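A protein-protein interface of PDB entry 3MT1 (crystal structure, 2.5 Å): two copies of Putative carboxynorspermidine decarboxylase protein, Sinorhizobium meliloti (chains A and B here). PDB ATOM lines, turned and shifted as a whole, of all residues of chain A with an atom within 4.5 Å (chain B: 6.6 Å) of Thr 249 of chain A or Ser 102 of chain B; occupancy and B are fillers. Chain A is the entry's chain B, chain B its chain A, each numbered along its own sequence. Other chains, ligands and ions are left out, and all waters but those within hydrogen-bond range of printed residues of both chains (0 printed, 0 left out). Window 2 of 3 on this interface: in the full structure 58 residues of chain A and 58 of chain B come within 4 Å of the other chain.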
ATOM      1  N   VAL A 246      30.571  35.380 -15.400  1.00  0.00           N
ATOM      2  CA  VAL A 246      30.273  34.028 -15.882  1.00  0.00           C
ATOM      3  C   VAL A 246      28.844  33.714 -15.510  1.00  0.00           C
ATOM      4  O   VAL A 246      28.412  34.012 -14.400  1.00  0.00           O
ATOM      5  CB  VAL A 246      31.214  33.000 -15.279  1.00  0.00           C
ATOM      6  CG1 VAL A 246      30.751  31.570 -15.567  1.00  0.00           C
ATOM      7  CG2 VAL A 246      32.629  33.248 -15.800  1.00  0.00           C
ATOM      8  N   ASP A 248      27.248  30.544 -16.893  1.00  0.00           N
ATOM      9  CA  ASP A 248      27.110  29.100 -16.875  1.00  0.00           C
ATOM     10  C   ASP A 248      28.438  28.429 -17.123  1.00  0.00           C
ATOM     11  O   ASP A 248      29.345  28.990 -17.730  1.00  0.00           O
ATOM     12  CB  ASP A 248      26.083  28.607 -17.893  1.00  0.00           C
ATOM     13  CG  ASP A 248      25.417  27.298 -17.465  1.00  0.00           C
ATOM     14  OD1 ASP A 248      25.344  27.001 -16.233  1.00  0.00           O
ATOM     15  OD2 ASP A 248      24.953  26.567 -18.373  1.00  0.00           O
ATOM     16  N   THR A 249      28.534  27.204 -16.637  1.00  0.00           N
ATOM     17  CA  THR A 249      29.751  26.436 -16.724  1.00  0.00           C
ATOM     18  C   THR A 249      29.397  25.108 -17.356  1.00  0.00           C
ATOM     19  O   THR A 249      28.301  24.615 -17.159  1.00  0.00           O
ATOM     20  CB  THR A 249      30.352  26.342 -15.328  1.00  0.00           C
ATOM     21  OG1 THR A 249      31.271  27.440 -15.187  1.00  0.00           O
ATOM     22  CG2 THR A 249      31.043  25.025 -15.082  1.00  0.00           C
ATOM     23  N   LEU A 250      30.295  24.559 -18.159  1.00  0.00           N
ATOM     24  CA  LEU A 250      29.976  23.372 -18.943  1.00  0.00           C
ATOM     25  C   LEU A 250      31.192  22.527 -19.231  1.00  0.00           C
ATOM     26  O   LEU A 250      32.288  23.044 -19.422  1.00  0.00           O
ATOM     27  CB  LEU A 250      29.327  23.762 -20.286  1.00  0.00           C
ATOM     28  CG  LEU A 250      27.899  24.316 -20.312  1.00  0.00           C
ATOM     29  CD1 LEU A 250      27.550  24.813 -21.703  1.00  0.00           C
ATOM     30  CD2 LEU A 250      26.882  23.267 -19.821  1.00  0.00           C
ATOM     31  N   LEU A 256      34.279  24.914 -20.605  1.00  0.00           N
ATOM     32  CA  LEU A 256      33.624  26.064 -21.222  1.00  0.00           C
ATOM     33  C   LEU A 256      32.951  26.951 -20.196  1.00  0.00           C
ATOM     34  O   LEU A 256      32.332  26.454 -19.256  1.00  0.00           O
ATOM     35  CB  LEU A 256      32.575  25.609 -22.229  1.00  0.00           C
ATOM     36  CG  LEU A 256      33.076  25.079 -23.568  1.00  0.00           C
ATOM     37  CD1 LEU A 256      31.998  24.203 -24.206  1.00  0.00           C
ATOM     38  CD2 LEU A 256      33.435  26.232 -24.488  1.00  0.00           C
ATOM     39  N   LEU A 310      36.330  28.189 -12.442  1.00  0.00           N
ATOM     40  CA  LEU A 310      35.381  29.283 -12.602  1.00  0.00           C
ATOM     41  C   LEU A 310      33.969  28.892 -12.184  1.00  0.00           C
ATOM     42  O   LEU A 310      33.486  27.797 -12.508  1.00  0.00           O
ATOM     43  CB  LEU A 310      35.341  29.761 -14.057  1.00  0.00           C
ATOM     44  CG  LEU A 310      36.522  30.520 -14.631  1.00  0.00           C
ATOM     45  CD1 LEU A 310      36.177  30.888 -16.064  1.00  0.00           C
ATOM     46  CD2 LEU A 310      36.865  31.765 -13.796  1.00  0.00           C
ATOM     47  N   VAL A 312      29.776  30.219 -11.724  1.00  0.00           N
ATOM     48  CA  VAL A 312      28.730  31.181 -12.041  1.00  0.00           C
ATOM     49  C   VAL A 312      28.819  32.374 -11.059  1.00  0.00           C
ATOM     50  O   VAL A 312      28.816  32.181  -9.854  1.00  0.00           O
ATOM     51  CB  VAL A 312      27.322  30.506 -11.990  1.00  0.00           C
ATOM     52  CG1 VAL A 312      26.177  31.546 -12.161  1.00  0.00           C
ATOM     53  CG2 VAL A 312      27.209  29.379 -13.018  1.00  0.00           C
ATOM     54  N   SER B 100      20.998  24.333 -20.829  1.00  0.00           N
ATOM     55  CA  SER B 100      21.590  23.205 -20.103  1.00  0.00           C
ATOM     56  C   SER B 100      20.816  22.831 -18.830  1.00  0.00           C
ATOM     57  O   SER B 100      19.906  23.555 -18.407  1.00  0.00           O
ATOM     58  CB  SER B 100      23.045  23.525 -19.757  1.00  0.00           C
ATOM     59  OG  SER B 100      23.105  24.550 -18.779  1.00  0.00           O
ATOM     60  N   ILE B 101      21.222  21.715 -18.214  1.00  0.00           N
ATOM     61  CA  ILE B 101      20.636  21.258 -16.979  1.00  0.00           C
ATOM     62  C   ILE B 101      21.043  22.197 -15.869  1.00  0.00           C
ATOM     63  O   ILE B 101      20.234  22.512 -15.007  1.00  0.00           O
ATOM     64  CB  ILE B 101      21.088  19.827 -16.590  1.00  0.00           C
ATOM     65  CG1 ILE B 101      20.967  18.820 -17.760  1.00  0.00           C
ATOM     66  CG2 ILE B 101      20.311  19.315 -15.363  1.00  0.00           C
ATOM     67  CD1 ILE B 101      19.596  18.289 -18.025  1.00  0.00           C
ATOM     68  N   SER B 102      22.288  22.654 -15.865  1.00  0.00           N
ATOM     69  CA  SER B 102      22.715  23.501 -14.743  1.00  0.00           C
ATOM     70  C   SER B 102      21.871  24.755 -14.700  1.00  0.00           C
ATOM     71  O   SER B 102      21.354  25.115 -13.630  1.00  0.00           O
ATOM     72  CB  SER B 102      24.199  23.831 -14.799  1.00  0.00           C
ATOM     73  OG  SER B 102      24.577  24.091 -16.129  1.00  0.00           O
ATOM     74  N   GLN B 103      21.721  25.377 -15.874  1.00  0.00           N
ATOM     75  CA  GLN B 103      20.788  26.490 -16.115  1.00  0.00           C
ATOM     76  C   GLN B 103      19.350  26.099 -15.786  1.00  0.00           C
ATOM     77  O   GLN B 103      18.651  26.823 -15.073  1.00  0.00           O
ATOM     78  CB  GLN B 103      20.840  26.950 -17.586  1.00  0.00           C
ATOM     79  CG  GLN B 103      21.952  27.915 -17.939  1.00  0.00           C
ATOM     80  CD  GLN B 103      21.529  29.333 -17.758  1.00  0.00           C
ATOM     81  OE1 GLN B 103      20.593  29.816 -18.422  1.00  0.00           O
ATOM     82  NE2 GLN B 103      22.212  30.037 -16.852  1.00  0.00           N
ATOM     83  N   LEU B 104      18.904  24.950 -16.303  1.00  0.00           N
ATOM     84  CA  LEU B 104      17.576  24.458 -15.933  1.00  0.00           C
ATOM     85  C   LEU B 104      17.455  24.393 -14.412  1.00  0.00           C
ATOM     86  O   LEU B 104      16.544  24.973 -13.825  1.00  0.00           O
ATOM     87  CB  LEU B 104      17.281  23.090 -16.543  1.00  0.00           C
ATOM     88  CG  LEU B 104      15.973  22.484 -16.031  1.00  0.00           C
ATOM     89  CD1 LEU B 104      14.734  23.255 -16.536  1.00  0.00           C
ATOM     90  CD2 LEU B 104      15.886  21.006 -16.408  1.00  0.00           C
ATOM     91  N   GLU B 105      18.393  23.721 -13.765  1.00  0.00           N
ATOM     92  CA  GLU B 105      18.316  23.576 -12.315  1.00  0.00           C
ATOM     93  C   GLU B 105      18.372  24.922 -11.607  1.00  0.00           C
ATOM     94  O   GLU B 105      17.653  25.144 -10.645  1.00  0.00           O
ATOM     95  CB  GLU B 105      19.400  22.642 -11.780  1.00  0.00           C
ATOM     96  CG  GLU B 105      19.169  21.188 -12.136  1.00  0.00           C
ATOM     97  CD  GLU B 105      20.398  20.322 -11.867  1.00  0.00           C
ATOM     98  OE1 GLU B 105      21.520  20.893 -11.669  1.00  0.00           O
ATOM     99  OE2 GLU B 105      20.230  19.072 -11.860  1.00  0.00           O
ATOM    100  N   ARG B 106      19.204  25.833 -12.084  1.00  0.00           N
ATOM    101  CA  ARG B 106      19.273  27.120 -11.408  1.00  0.00           C
ATOM    102  C   ARG B 106      17.970  27.951 -11.506  1.00  0.00           C
ATOM    103  O   ARG B 106      17.667  28.691 -10.585  1.00  0.00           O
ATOM    104  CB  ARG B 106      20.521  27.892 -11.851  1.00  0.00           C
ATOM    105  CG  ARG B 106      20.584  29.374 -11.437  1.00  0.00           C
ATOM    106  CD  ARG B 106      21.903  30.017 -11.865  1.00  0.00           C
ATOM    107  NE  ARG B 106      22.953  29.585 -10.951  1.00  0.00           N
ATOM    108  CZ  ARG B 106      23.415  30.315  -9.945  1.00  0.00           C
ATOM    109  NH1 ARG B 106      22.955  31.540  -9.738  1.00  0.00           N
ATOM    110  NH2 ARG B 106      24.350  29.819  -9.155  1.00  0.00           N
ATOM    111  N   PHE B 107      17.175  27.816 -12.577  1.00  0.00           N
ATOM    112  CA  PHE B 107      16.055  28.763 -12.762  1.00  0.00           C
ATOM    113  C   PHE B 107      14.649  28.199 -12.809  1.00  0.00           C
ATOM    114  O   PHE B 107      13.684  28.977 -12.899  1.00  0.00           O
ATOM    115  CB  PHE B 107      16.248  29.637 -14.002  1.00  0.00           C
ATOM    116  CG  PHE B 107      17.523  30.402 -14.006  1.00  0.00           C
ATOM    117  CD1 PHE B 107      17.754  31.401 -13.048  1.00  0.00           C
ATOM    118  CD2 PHE B 107      18.494  30.137 -14.959  1.00  0.00           C
ATOM    119  CE1 PHE B 107      18.938  32.140 -13.045  1.00  0.00           C
ATOM    120  CE2 PHE B 107      19.695  30.851 -14.946  1.00  0.00           C
ATOM    121  CZ  PHE B 107      19.909  31.870 -13.989  1.00  0.00           C
ATOM    122  N   GLU B 143      21.877  19.671 -24.368  1.00  0.00           N
ATOM    123  CA  GLU B 143      22.328  18.403 -23.787  1.00  0.00           C
ATOM    124  C   GLU B 143      22.286  17.245 -24.801  1.00  0.00           C
ATOM    125  O   GLU B 143      21.536  17.283 -25.759  1.00  0.00           O
ATOM    126  CB  GLU B 143      21.508  18.067 -22.532  1.00  0.00           C
ATOM    127  CG  GLU B 143      21.663  19.065 -21.354  1.00  0.00           C
ATOM    128  CD  GLU B 143      23.044  19.050 -20.655  1.00  0.00           C
ATOM    129  OE1 GLU B 143      23.837  18.099 -20.879  1.00  0.00           O
ATOM    130  OE2 GLU B 143      23.332  20.003 -19.879  1.00  0.00           O
ATOM    131  N   LYS B 148      21.534  11.417 -18.407  1.00  0.00           N
ATOM    132  CA  LYS B 148      21.554  12.666 -17.644  1.00  0.00           C
ATOM    133  C   LYS B 148      20.252  13.464 -17.748  1.00  0.00           C
ATOM    134  O   LYS B 148      19.774  13.982 -16.753  1.00  0.00           O
ATOM    135  CB  LYS B 148      22.750  13.521 -18.067  1.00  0.00           C
ATOM    136  CG  LYS B 148      23.138  14.607 -17.071  1.00  0.00           C
ATOM    137  CD  LYS B 148      24.666  14.710 -16.967  1.00  0.00           C
ATOM    138  CE  LYS B 148      25.135  16.089 -16.483  1.00  0.00           C
ATOM    139  NZ  LYS B 148      24.658  17.178 -17.405  1.00  0.00           N
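The side-chain carboxylate of Asp 248 of chain A sits at hydrogen-bond distance from the side-chain hydroxyl of Ser 100 of chain B, 2.8 Å away. The side-chain hydroxyl (OG) of Ser 102 of chain B sits at hydrogen-bond distance from the side-chain carboxylate (OD1) of Asp 248 of chain A (3.0 Å).
The side-chain hydroxyl (OG) of Ser 100 of chain B lies within hydrogen-bond range of the side-chain hydroxyl (OG) of Ser 102 of chain B (3.1 Å). The side-chain hydroxyl of Ser 100 of chain B lies within hydrogen-bond range of the backbone NH of Gln 103 of chain B (3.3 Å). OG1 of Thr 249 of chain A is in hydrogen-bond range of O of Leu 310 of chain A, 3.5 Å away. The backbone NH (N) of Leu 256 of chain A is in hydrogen-bond range of the backbone carbonyl oxygen (O) of Leu 250 of chain A (3.0 Å).
Asp 248 of chain A touches Gln 103 of chain B (OD2 to CG, 3.3 Å). O of Thr 249 of chain A touches OG of Ser 102 of chain B (3.9 Å). Ser 100 of chain B touches Leu 250 of chain A. CG1 of Val 312 of chain A touches CZ of Arg 106 of chain B, 3.7 Å away.
Thr 249 of chain A touches one residue of chain B. Of chain A, only Asp 248 (3.0 Å) and Thr 249 (3.9 Å) come within 4 Å of Ser 102 of chain B. Printed residues of chain A within 4 Å of Ser 100 of chain B: Asp 248 (2.8 Å) and Leu 250 (3.8 Å). Printed residues of chain B within 4 Å of Val 312 of chain A: Arg 106. Of the printed residues of chain B, Asp 248 of chain A touches Ser 100 (2.8 Å), Ser 102 (3.0 Å) and Gln 103 (3.3 Å). Of the printed residues of chain A, Gln 103 of chain B touches Asp 248. The nearest residue of chain B that does not touch Thr 249 of chain A is Ser 100 of chain B (5.4 Å). The nearest residue of chain A that does not touch Ser 102 of chain B is Leu 250 of chain A (4.4 Å).
Printed residues of chain A that touch a printed residue of chain B: Asp 248, Thr 249, Leu 250 and Val 312. Hydrophobic or aromatic side chains of chain A that line the printed part of chain B: Leu 250 and Val 312. Among the printed residues, no Asp or Glu carboxylate lies within 4 Å of a Lys or Arg side-chain nitrogen of the other chain.
No position is printed for both chains.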
